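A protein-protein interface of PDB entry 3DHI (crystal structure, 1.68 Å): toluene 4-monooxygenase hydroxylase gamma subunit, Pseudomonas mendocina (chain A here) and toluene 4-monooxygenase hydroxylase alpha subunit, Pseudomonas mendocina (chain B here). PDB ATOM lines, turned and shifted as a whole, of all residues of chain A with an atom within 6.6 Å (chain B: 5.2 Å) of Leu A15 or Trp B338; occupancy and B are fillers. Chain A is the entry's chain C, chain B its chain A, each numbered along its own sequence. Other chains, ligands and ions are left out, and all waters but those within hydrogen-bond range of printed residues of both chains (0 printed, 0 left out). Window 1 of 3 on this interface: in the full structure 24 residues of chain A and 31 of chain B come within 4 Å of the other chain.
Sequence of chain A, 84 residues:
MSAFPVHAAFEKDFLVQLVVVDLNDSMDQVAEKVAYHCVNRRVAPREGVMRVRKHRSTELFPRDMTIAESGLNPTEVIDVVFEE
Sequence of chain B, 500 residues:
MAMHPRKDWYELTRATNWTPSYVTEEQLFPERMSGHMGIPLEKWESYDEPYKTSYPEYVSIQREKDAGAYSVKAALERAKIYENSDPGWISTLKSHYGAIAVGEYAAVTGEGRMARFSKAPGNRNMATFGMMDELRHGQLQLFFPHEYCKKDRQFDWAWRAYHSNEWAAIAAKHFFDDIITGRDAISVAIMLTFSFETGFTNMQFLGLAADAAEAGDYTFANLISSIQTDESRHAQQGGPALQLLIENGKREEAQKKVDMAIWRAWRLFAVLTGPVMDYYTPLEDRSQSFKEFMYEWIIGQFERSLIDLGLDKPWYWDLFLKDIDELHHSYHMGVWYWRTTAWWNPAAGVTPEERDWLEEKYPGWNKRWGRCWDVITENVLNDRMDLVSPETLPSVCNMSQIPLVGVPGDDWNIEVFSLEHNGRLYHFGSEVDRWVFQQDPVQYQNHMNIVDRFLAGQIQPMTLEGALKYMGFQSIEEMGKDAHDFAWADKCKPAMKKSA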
ATOM      1  N   ALA A   8      27.757  14.306   5.839  1.00  0.00           N
ATOM      2  CA  ALA A   8      28.420  15.349   5.077  1.00  0.00           C
ATOM      3  C   ALA A   8      28.416  15.110   3.573  1.00  0.00           C
ATOM      4  O   ALA A   8      28.694  14.004   3.118  1.00  0.00           O
ATOM      5  CB  ALA A   8      29.879  15.542   5.616  1.00  0.00           C
ATOM      6  N   ALA A   9      28.118  16.163   2.809  1.00  0.00           N
ATOM      7  CA  ALA A   9      28.163  16.124   1.352  1.00  0.00           C
ATOM      8  C   ALA A   9      29.323  16.998   0.901  1.00  0.00           C
ATOM      9  O   ALA A   9      29.321  18.219   1.154  1.00  0.00           O
ATOM     10  CB  ALA A   9      26.839  16.650   0.763  1.00  0.00           C
ATOM     11  N   PHE A  10      30.311  16.373   0.269  1.00  0.00           N
ATOM     12  CA  PHE A  10      31.480  17.087  -0.220  1.00  0.00           C
ATOM     13  C   PHE A  10      31.251  17.581  -1.640  1.00  0.00           C
ATOM     14  O   PHE A  10      30.692  16.847  -2.476  1.00  0.00           O
ATOM     15  CB  PHE A  10      32.711  16.177  -0.191  1.00  0.00           C
ATOM     16  CG  PHE A  10      34.002  16.937  -0.279  1.00  0.00           C
ATOM     17  CD1 PHE A  10      34.554  17.252  -1.513  1.00  0.00           C
ATOM     18  CD2 PHE A  10      34.619  17.385   0.882  1.00  0.00           C
ATOM     19  CE1 PHE A  10      35.730  17.995  -1.597  1.00  0.00           C
ATOM     20  CE2 PHE A  10      35.791  18.124   0.820  1.00  0.00           C
ATOM     21  CZ  PHE A  10      36.345  18.431  -0.420  1.00  0.00           C
ATOM     22  N   ASP A  13      31.231  15.451  -5.182  1.00  0.00           N
ATOM     23  CA  ASP A  13      31.064  14.023  -4.901  1.00  0.00           C
ATOM     24  C   ASP A  13      29.619  13.607  -5.236  1.00  0.00           C
ATOM     25  O   ASP A  13      28.788  14.452  -5.574  1.00  0.00           O
ATOM     26  CB  ASP A  13      31.352  13.758  -3.422  1.00  0.00           C
ATOM     27  CG  ASP A  13      31.791  12.327  -3.139  1.00  0.00           C
ATOM     28  OD1 ASP A  13      31.816  11.471  -4.073  1.00  0.00           O
ATOM     29  OD2 ASP A  13      32.109  12.060  -1.961  1.00  0.00           O
ATOM     30  N   PHE A  14      29.351  12.309  -5.179  1.00  0.00           N
ATOM     31  CA  PHE A  14      28.036  11.781  -5.606  1.00  0.00           C
ATOM     32  C   PHE A  14      27.103  11.438  -4.450  1.00  0.00           C
ATOM     33  O   PHE A  14      25.944  11.072  -4.688  1.00  0.00           O
ATOM     34  CB  PHE A  14      28.216  10.546  -6.511  1.00  0.00           C
ATOM     35  CG  PHE A  14      28.402   9.258  -5.752  1.00  0.00           C
ATOM     36  CD1 PHE A  14      27.315   8.395  -5.512  1.00  0.00           C
ATOM     37  CD2 PHE A  14      29.642   8.918  -5.242  1.00  0.00           C
ATOM     38  CE1 PHE A  14      27.475   7.224  -4.792  1.00  0.00           C
ATOM     39  CE2 PHE A  14      29.824   7.731  -4.506  1.00  0.00           C
ATOM     40  CZ  PHE A  14      28.724   6.874  -4.284  1.00  0.00           C
ATOM     41  N   LEU A  15      27.586  11.544  -3.214  1.00  0.00           N
ATOM     42  CA  LEU A  15      26.803  11.120  -2.064  1.00  0.00           C
ATOM     43  C   LEU A  15      27.046  11.909  -0.778  1.00  0.00           C
ATOM     44  O   LEU A  15      27.920  12.791  -0.713  1.00  0.00           O
ATOM     45  CB  LEU A  15      26.996   9.616  -1.824  1.00  0.00           C
ATOM     46  CG  LEU A  15      28.099   9.194  -0.852  1.00  0.00           C
ATOM     47  CD1 LEU A  15      28.007   7.709  -0.596  1.00  0.00           C
ATOM     48  CD2 LEU A  15      29.476   9.550  -1.397  1.00  0.00           C
ATOM     49  N   VAL A  16      26.244  11.575   0.226  1.00  0.00           N
ATOM     50  CA  VAL A  16      26.375  12.077   1.576  1.00  0.00           C
ATOM     51  C   VAL A  16      26.910  10.913   2.405  1.00  0.00           C
ATOM     52  O   VAL A  16      26.439   9.774   2.272  1.00  0.00           O
ATOM     53  CB  VAL A  16      24.994  12.528   2.146  1.00  0.00           C
ATOM     54  CG1 VAL A  16      25.144  13.125   3.546  1.00  0.00           C
ATOM     55  CG2 VAL A  16      24.366  13.560   1.218  1.00  0.00           C
ATOM     56  N   GLN A  17      27.882  11.187   3.276  1.00  0.00           N
ATOM     57  CA  GLN A  17      28.495  10.134   4.071  1.00  0.00           C
ATOM     58  C   GLN A  17      28.458  10.451   5.549  1.00  0.00           C
ATOM     59  O   GLN A  17      28.458  11.635   5.945  1.00  0.00           O
ATOM     60  CB  GLN A  17      29.968   9.908   3.672  1.00  0.00           C
ATOM     61  CG  GLN A  17      30.181   9.379   2.284  1.00  0.00           C
ATOM     62  CD  GLN A  17      31.654   9.310   1.937  1.00  0.00           C
ATOM     63  OE1 GLN A  17      32.342  10.344   1.830  1.00  0.00           O
ATOM     64  NE2 GLN A  17      32.143   8.101   1.755  1.00  0.00           N
ATOM     65  N   HIS A  37      37.546  11.343   3.113  1.00  0.00           N
ATOM     66  CA  HIS A  37      36.719  10.298   2.550  1.00  0.00           C
ATOM     67  C   HIS A  37      36.243  10.583   1.120  1.00  0.00           C
ATOM     68  O   HIS A  37      35.402   9.842   0.598  1.00  0.00           O
ATOM     69  CB  HIS A  37      35.513  10.060   3.462  1.00  0.00           C
ATOM     70  CG  HIS A  37      35.873   9.531   4.812  1.00  0.00           C
ATOM     71  ND1 HIS A  37      36.308   8.239   5.014  1.00  0.00           N
ATOM     72  CD2 HIS A  37      35.858  10.120   6.032  1.00  0.00           C
ATOM     73  CE1 HIS A  37      36.535   8.053   6.303  1.00  0.00           C
ATOM     74  NE2 HIS A  37      36.272   9.178   6.943  1.00  0.00           N
ATOM     75  N   CYS A  38      36.769  11.633   0.489  1.00  0.00           N
ATOM     76  CA  CYS A  38      36.252  12.103  -0.806  1.00  0.00           C
ATOM     77  C   CYS A  38      37.354  12.500  -1.771  1.00  0.00           C
ATOM     78  O   CYS A  38      37.418  12.003  -2.903  1.00  0.00           O
ATOM     79  CB  CYS A  38      35.295  13.296  -0.616  1.00  0.00           C
ATOM     80  SG  CYS A  38      33.975  13.065   0.644  1.00  0.00           S
ATOM     81  N   ARG A  42      36.928  10.094  -5.034  1.00  0.00           N
ATOM     82  CA  ARG A  42      35.977  10.365  -6.102  1.00  0.00           C
ATOM     83  C   ARG A  42      35.988  11.815  -6.553  1.00  0.00           C
ATOM     84  O   ARG A  42      35.316  12.154  -7.522  1.00  0.00           O
ATOM     85  CB  ARG A  42      34.565   9.951  -5.673  1.00  0.00           C
ATOM     86  CG  ARG A  42      34.448   8.445  -5.355  1.00  0.00           C
ATOM     87  CD  ARG A  42      33.123   8.095  -4.700  1.00  0.00           C
ATOM     88  NE  ARG A  42      32.926   8.926  -3.519  1.00  0.00           N
ATOM     89  CZ  ARG A  42      33.350   8.614  -2.300  1.00  0.00           C
ATOM     90  NH1 ARG A  42      33.153   9.462  -1.303  1.00  0.00           N
ATOM     91  NH2 ARG A  42      33.950   7.449  -2.074  1.00  0.00           N
ATOM     92  N   TRP B 167      22.551  -4.771   3.626  1.00  0.00           N
ATOM     93  CA  TRP B 167      21.838  -3.482   3.459  1.00  0.00           C
ATOM     94  C   TRP B 167      20.791  -3.559   2.336  1.00  0.00           C
ATOM     95  O   TRP B 167      19.689  -2.991   2.455  1.00  0.00           O
ATOM     96  CB  TRP B 167      22.828  -2.319   3.213  1.00  0.00           C
ATOM     97  CG  TRP B 167      23.508  -2.361   1.882  1.00  0.00           C
ATOM     98  CD1 TRP B 167      24.720  -2.931   1.596  1.00  0.00           C
ATOM     99  CD2 TRP B 167      23.016  -1.818   0.644  1.00  0.00           C
ATOM    100  NE1 TRP B 167      25.014  -2.772   0.263  1.00  0.00           N
ATOM    101  CE2 TRP B 167      23.979  -2.105  -0.347  1.00  0.00           C
ATOM    102  CE3 TRP B 167      21.856  -1.112   0.277  1.00  0.00           C
ATOM    103  CZ2 TRP B 167      23.825  -1.707  -1.679  1.00  0.00           C
ATOM    104  CZ3 TRP B 167      21.696  -0.732  -1.037  1.00  0.00           C
ATOM    105  CH2 TRP B 167      22.671  -1.027  -2.009  1.00  0.00           C
ATOM    106  N   MET B 333      27.283   3.744  -8.704  1.00  0.00           N
ATOM    107  CA  MET B 333      28.553   4.205  -8.123  1.00  0.00           C
ATOM    108  C   MET B 333      28.682   3.784  -6.665  1.00  0.00           C
ATOM    109  O   MET B 333      29.758   3.350  -6.233  1.00  0.00           O
ATOM    110  CB  MET B 333      28.704   5.723  -8.261  1.00  0.00           C
ATOM    111  CG  MET B 333      30.108   6.245  -7.910  1.00  0.00           C
ATOM    112  SD  MET B 333      30.251   7.951  -8.457  1.00  0.00           S
ATOM    113  CE  MET B 333      30.360   7.755 -10.225  1.00  0.00           C
ATOM    114  N   GLY B 334      27.592   3.913  -5.905  1.00  0.00           N
ATOM    115  CA  GLY B 334      27.573   3.587  -4.488  1.00  0.00           C
ATOM    116  C   GLY B 334      27.725   2.103  -4.256  1.00  0.00           C
ATOM    117  O   GLY B 334      28.490   1.673  -3.389  1.00  0.00           O
ATOM    118  N   VAL B 335      26.973   1.305  -5.015  1.00  0.00           N
ATOM    119  CA  VAL B 335      27.050  -0.144  -4.911  1.00  0.00           C
ATOM    120  C   VAL B 335      28.455  -0.622  -5.300  1.00  0.00           C
ATOM    121  O   VAL B 335      28.994  -1.516  -4.665  1.00  0.00           O
ATOM    122  CB  VAL B 335      25.992  -0.824  -5.810  1.00  0.00           C
ATOM    123  CG1 VAL B 335      26.245  -2.325  -5.950  1.00  0.00           C
ATOM    124  CG2 VAL B 335      24.568  -0.590  -5.233  1.00  0.00           C
ATOM    125  N   TRP B 336      29.048  -0.006  -6.319  1.00  0.00           N
ATOM    126  CA  TRP B 336      30.392  -0.442  -6.741  1.00  0.00           C
ATOM    127  C   TRP B 336      31.442  -0.017  -5.699  1.00  0.00           C
ATOM    128  O   TRP B 336      32.270  -0.822  -5.281  1.00  0.00           O
ATOM    129  CB  TRP B 336      30.780   0.093  -8.124  1.00  0.00           C
ATOM    130  CG  TRP B 336      32.109  -0.499  -8.570  1.00  0.00           C
ATOM    131  CD1 TRP B 336      32.300  -1.652  -9.276  1.00  0.00           C
ATOM    132  CD2 TRP B 336      33.421   0.042  -8.316  1.00  0.00           C
ATOM    133  NE1 TRP B 336      33.653  -1.874  -9.476  1.00  0.00           N
ATOM    134  CE2 TRP B 336      34.358  -0.845  -8.900  1.00  0.00           C
ATOM    135  CE3 TRP B 336      33.889   1.185  -7.647  1.00  0.00           C
ATOM    136  CZ2 TRP B 336      35.735  -0.615  -8.853  1.00  0.00           C
ATOM    137  CZ3 TRP B 336      35.265   1.418  -7.600  1.00  0.00           C
ATOM    138  CH2 TRP B 336      36.168   0.509  -8.191  1.00  0.00           C
ATOM    139  N   TYR B 337      31.413   1.242  -5.273  1.00  0.00           N
ATOM    140  CA  TYR B 337      32.418   1.659  -4.277  1.00  0.00           C
ATOM    141  C   TYR B 337      32.323   0.835  -2.986  1.00  0.00           C
ATOM    142  O   TYR B 337      33.346   0.442  -2.434  1.00  0.00           O
ATOM    143  CB  TYR B 337      32.303   3.147  -3.983  1.00  0.00           C
ATOM    144  CG  TYR B 337      33.597   3.725  -3.451  1.00  0.00           C
ATOM    145  CD1 TYR B 337      34.611   4.113  -4.320  1.00  0.00           C
ATOM    146  CD2 TYR B 337      33.794   3.867  -2.080  1.00  0.00           C
ATOM    147  CE1 TYR B 337      35.815   4.633  -3.831  1.00  0.00           C
ATOM    148  CE2 TYR B 337      34.981   4.396  -1.580  1.00  0.00           C
ATOM    149  CZ  TYR B 337      35.978   4.768  -2.470  1.00  0.00           C
ATOM    150  OH  TYR B 337      37.153   5.297  -1.967  1.00  0.00           O
ATOM    151  N   TRP B 338      31.093   0.564  -2.529  1.00  0.00           N
ATOM    152  CA  TRP B 338      30.856  -0.247  -1.348  1.00  0.00           C
ATOM    153  C   TRP B 338      30.590  -1.728  -1.686  1.00  0.00           C
ATOM    154  O   TRP B 338      29.893  -2.431  -0.946  1.00  0.00           O
ATOM    155  CB  TRP B 338      29.712   0.346  -0.507  1.00  0.00           C
ATOM    156  CG  TRP B 338      30.168   1.448   0.414  1.00  0.00           C
ATOM    157  CD1 TRP B 338      30.482   1.329   1.736  1.00  0.00           C
ATOM    158  CD2 TRP B 338      30.342   2.824   0.076  1.00  0.00           C
ATOM    159  NE1 TRP B 338      30.869   2.561   2.242  1.00  0.00           N
ATOM    160  CE2 TRP B 338      30.800   3.490   1.243  1.00  0.00           C
ATOM    161  CE3 TRP B 338      30.199   3.556  -1.109  1.00  0.00           C
ATOM    162  CZ2 TRP B 338      31.082   4.873   1.263  1.00  0.00           C
ATOM    163  CZ3 TRP B 338      30.472   4.932  -1.090  1.00  0.00           C
ATOM    164  CH2 TRP B 338      30.912   5.572   0.088  1.00  0.00           C
ATOM    165  N   ARG B 339      31.192  -2.189  -2.777  1.00  0.00           N
ATOM    166  CA  ARG B 339      30.937  -3.547  -3.306  1.00  0.00           C
ATOM    167  C   ARG B 339      31.148  -4.633  -2.254  1.00  0.00           C
ATOM    168  O   ARG B 339      30.457  -5.664  -2.249  1.00  0.00           O
ATOM    169  CB  ARG B 339      31.802  -3.819  -4.530  1.00  0.00           C
ATOM    170  CG  ARG B 339      33.332  -3.688  -4.259  1.00  0.00           C
ATOM    171  CD  ARG B 339      34.070  -3.419  -5.548  1.00  0.00           C
ATOM    172  NE  ARG B 339      35.487  -3.255  -5.247  1.00  0.00           N
ATOM    173  CZ  ARG B 339      36.029  -2.109  -4.839  1.00  0.00           C
ATOM    174  NH1 ARG B 339      37.334  -2.061  -4.561  1.00  0.00           N
ATOM    175  NH2 ARG B 339      35.284  -1.013  -4.708  1.00  0.00           N
ATOM    176  N   THR B 340      32.082  -4.407  -1.328  1.00  0.00           N
ATOM    177  CA  THR B 340      32.360  -5.439  -0.332  1.00  0.00           C
ATOM    178  C   THR B 340      31.144  -5.761   0.545  1.00  0.00           C
ATOM    179  O   THR B 340      31.095  -6.796   1.197  1.00  0.00           O
ATOM    180  CB  THR B 340      33.628  -5.085   0.527  1.00  0.00           C
ATOM    181  OG1 THR B 340      34.024  -6.254   1.263  1.00  0.00           O
ATOM    182  CG2 THR B 340      33.342  -3.950   1.452  1.00  0.00           C
ATOM    183  N   THR B 341      30.135  -4.899   0.511  1.00  0.00           N
ATOM    184  CA  THR B 341      28.912  -5.105   1.306  1.00  0.00           C
ATOM    185  C   THR B 341      27.796  -5.834   0.543  1.00  0.00           C
ATOM    186  O   THR B 341      26.748  -6.102   1.126  1.00  0.00           O
ATOM    187  CB  THR B 341      28.323  -3.751   1.828  1.00  0.00           C
ATOM    188  OG1 THR B 341      27.840  -2.952   0.741  1.00  0.00           O
ATOM    189  CG2 THR B 341      29.400  -2.983   2.630  1.00  0.00           C
ATOM    190  N   ALA B 342      28.025  -6.102  -0.740  1.00  0.00           N
ATOM    191  CA  ALA B 342      27.030  -6.772  -1.616  1.00  0.00           C
ATOM    192  C   ALA B 342      27.365  -8.252  -1.675  1.00  0.00           C
ATOM    193  O   ALA B 342      28.535  -8.635  -1.451  1.00  0.00           O
ATOM    194  CB  ALA B 342      27.107  -6.188  -3.014  1.00  0.00           C
ATOM    195  N   PRO B 390      36.156   1.828   0.766  1.00  0.00           N
ATOM    196  CA  PRO B 390      35.685   2.840   1.712  1.00  0.00           C
ATOM    197  C   PRO B 390      36.142   2.630   3.150  1.00  0.00           C
ATOM    198  O   PRO B 390      36.357   1.491   3.605  1.00  0.00           O
ATOM    199  CB  PRO B 390      34.159   2.700   1.628  1.00  0.00           C
ATOM    200  CG  PRO B 390      33.962   1.221   1.376  1.00  0.00           C
ATOM    201  CD  PRO B 390      35.121   0.802   0.490  1.00  0.00           C
ATOM    202  N   THR B 392      34.359   4.613   5.552  1.00  0.00           N
ATOM    203  CA  THR B 392      33.200   5.029   6.320  1.00  0.00           C
ATOM    204  C   THR B 392      31.915   4.477   5.692  1.00  0.00           C
ATOM    205  O   THR B 392      31.970   3.775   4.671  1.00  0.00           O
ATOM    206  CB  THR B 392      33.137   6.567   6.487  1.00  0.00           C
ATOM    207  OG1 THR B 392      32.212   6.896   7.530  1.00  0.00           O
ATOM    208  CG2 THR B 392      32.744   7.283   5.177  1.00  0.00           C
ATOM    209  N   LEU B 393      30.787   4.799   6.314  1.00  0.00           N
ATOM    210  CA  LEU B 393      29.459   4.431   5.801  1.00  0.00           C
ATOM    211  C   LEU B 393      28.876   5.550   4.950  1.00  0.00           C
ATOM    212  O   LEU B 393      29.086   6.736   5.226  1.00  0.00           O
ATOM    213  CB  LEU B 393      28.483   4.148   6.947  1.00  0.00           C
ATOM    214  CG  LEU B 393      28.693   2.898   7.797  1.00  0.00           C
ATOM    215  CD1 LEU B 393      29.877   3.101   8.743  1.00  0.00           C
ATOM    216  CD2 LEU B 393      27.446   2.596   8.599  1.00  0.00           C
ATOM    217  N   PRO B 394      28.103   5.178   3.919  1.00  0.00           N
ATOM    218  CA  PRO B 394      27.284   6.190   3.277  1.00  0.00           C
ATOM    219  C   PRO B 394      26.113   6.522   4.192  1.00  0.00           C
ATOM    220  O   PRO B 394      25.701   5.682   5.005  1.00  0.00           O
ATOM    221  CB  PRO B 394      26.754   5.483   2.018  1.00  0.00           C
ATOM    222  CG  PRO B 394      26.893   4.025   2.275  1.00  0.00           C
ATOM    223  CD  PRO B 394      27.893   3.823   3.369  1.00  0.00           C
ATOM    224  N   PRO B 403      21.670   4.405   0.034  1.00  0.00           N
ATOM    225  CA  PRO B 403      22.467   5.649   0.118  1.00  0.00           C
ATOM    226  C   PRO B 403      21.825   6.949  -0.427  1.00  0.00           C
ATOM    227  O   PRO B 403      21.159   6.938  -1.469  1.00  0.00           O
ATOM    228  CB  PRO B 403      23.707   5.301  -0.709  1.00  0.00           C
ATOM    229  CG  PRO B 403      23.951   3.874  -0.344  1.00  0.00           C
ATOM    230  CD  PRO B 403      22.539   3.229  -0.185  1.00  0.00           C
ATOM    231  N   LEU B 404      22.065   8.053   0.283  1.00  0.00           N
ATOM    232  CA  LEU B 404      21.652   9.383  -0.139  1.00  0.00           C
ATOM    233  C   LEU B 404      22.616   9.910  -1.170  1.00  0.00           C
ATOM    234  O   LEU B 404      23.782  10.180  -0.851  1.00  0.00           O
ATOM    235  CB  LEU B 404      21.627  10.336   1.057  1.00  0.00           C
ATOM    236  CG  LEU B 404      20.677   9.918   2.171  1.00  0.00           C
ATOM    237  CD1 LEU B 404      20.834  10.799   3.401  1.00  0.00           C
ATOM    238  CD2 LEU B 404      19.231   9.965   1.644  1.00  0.00           C
ATOM    239  N   VAL B 405      22.130  10.066  -2.398  1.00  0.00           N
ATOM    240  CA  VAL B 405      22.994  10.450  -3.513  1.00  0.00           C
ATOM    241  C   VAL B 405      22.540  11.702  -4.243  1.00  0.00           C
ATOM    242  O   VAL B 405      21.469  12.256  -3.963  1.00  0.00           O
ATOM    243  CB  VAL B 405      23.143   9.294  -4.531  1.00  0.00           C
ATOM    244  CG1 VAL B 405      23.681   8.056  -3.846  1.00  0.00           C
ATOM    245  CG2 VAL B 405      21.778   8.988  -5.203  1.00  0.00           C
ATOM    246  N   GLY B 406      23.363  12.142  -5.188  1.00  0.00           N
ATOM    247  CA  GLY B 406      23.037  13.285  -6.028  1.00  0.00           C
ATOM    248  C   GLY B 406      23.836  13.233  -7.307  1.00  0.00           C
ATOM    249  O   GLY B 406      24.366  12.188  -7.677  1.00  0.00           O
ATOM    250  N   ILE B 414      23.275  17.998  -4.807  1.00  0.00           N
ATOM    251  CA  ILE B 414      22.792  16.941  -3.925  1.00  0.00           C
ATOM    252  C   ILE B 414      21.836  17.513  -2.883  1.00  0.00           C
ATOM    253  O   ILE B 414      22.072  18.602  -2.338  1.00  0.00           O
ATOM    254  CB  ILE B 414      23.978  16.145  -3.308  1.00  0.00           C
ATOM    255  CG1 ILE B 414      23.513  14.862  -2.609  1.00  0.00           C
ATOM    256  CG2 ILE B 414      24.792  17.003  -2.330  1.00  0.00           C
ATOM    257  CD1 ILE B 414      24.625  13.807  -2.489  1.00  0.00           C
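Of the 20 printed residues of chain B, 11 touch a printed residue of chain A.
Printed residues of chain B that touch a printed residue of chain A: Met B333, Gly B334, Tyr B337, Trp B338, Thr B392, Leu B393, Pro B394, Leu B404, Val B405, Gly B406 and Ile B414.
Hydrophobic or aromatic side chains of chain B within 4 Å of the printed part of chain A: Met B333, Tyr B337, Trp B338, Pro B394, Val B405 and Ile B414.
Among the printed residues, 18 pairs touch across the chains.
Met B333 touches Phe A14 (SD to CD2, 3.4 Å).
Phe A14 touches Val B405 (O to CA, 3.2 Å).
Leu A15 touches Trp B338.
Leu A15 touches Leu B404.
Ile B414 touches Val A16.
Trp B338 touches Gln A17 (CH2 to NE2, 3.3 Å).
Thr B392 touches Gln A17 (CG2 to NE2, 3.6 Å).
O of Leu B393 touches CA of Gln A17 (3.6 Å).
ND1 of His A37 touches CG2 of Thr B392 (3.7 Å).
Tyr B337 touches Arg A42 (CE2 to NH2, 3.3 Å).
The backbone carbonyl oxygen of His A37 sits at hydrogen-bond distance from the guanidinium group of Arg A42 (3.0 Å).
O of Trp B338 is in hydrogen-bond range of OG1 of Thr B341 (2.7 Å).
O of Thr B392 is in hydrogen-bond range of NE1 of Trp B338 (2.9 Å).
The side-chain sulfur (SG) of Cys A38 lies within hydrogen-bond range of the side-chain amide oxygen (OE1) of Gln A17.
OD1 of Asp A13 lies within salt-bridge range of NE of Arg A42 (2.8 Å).
The side-chain amide oxygen (OE1) of Gln A17 lies within hydrogen-bond range of the guanidinium group (NH1) of Arg A42, at 3.4 Å.
The backbone carbonyl oxygen (O) of Leu B404 sits at hydrogen-bond distance from the backbone NH (N) of Val A16, at 3.0 Å.
The backbone carbonyl oxygen of Phe A14 is in hydrogen-bond range of the backbone NH of Gly B406, 2.8 Å away.
Trp B167 touches none of the printed residues of chain A.
Printed residues of chain A within 4 Å of Thr B392: Gln A17 (3.6 Å) and His A37 (3.7 Å).
Of the printed residues of chain A, Ile B414 touches Ala A9 (3.7 Å), Phe A14 (3.7 Å), Leu A15 (3.5 Å) and Val A16 (3.7 Å).
The nearest residue of chain B that does not touch Leu A15 is Val B405 (4.1 Å).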
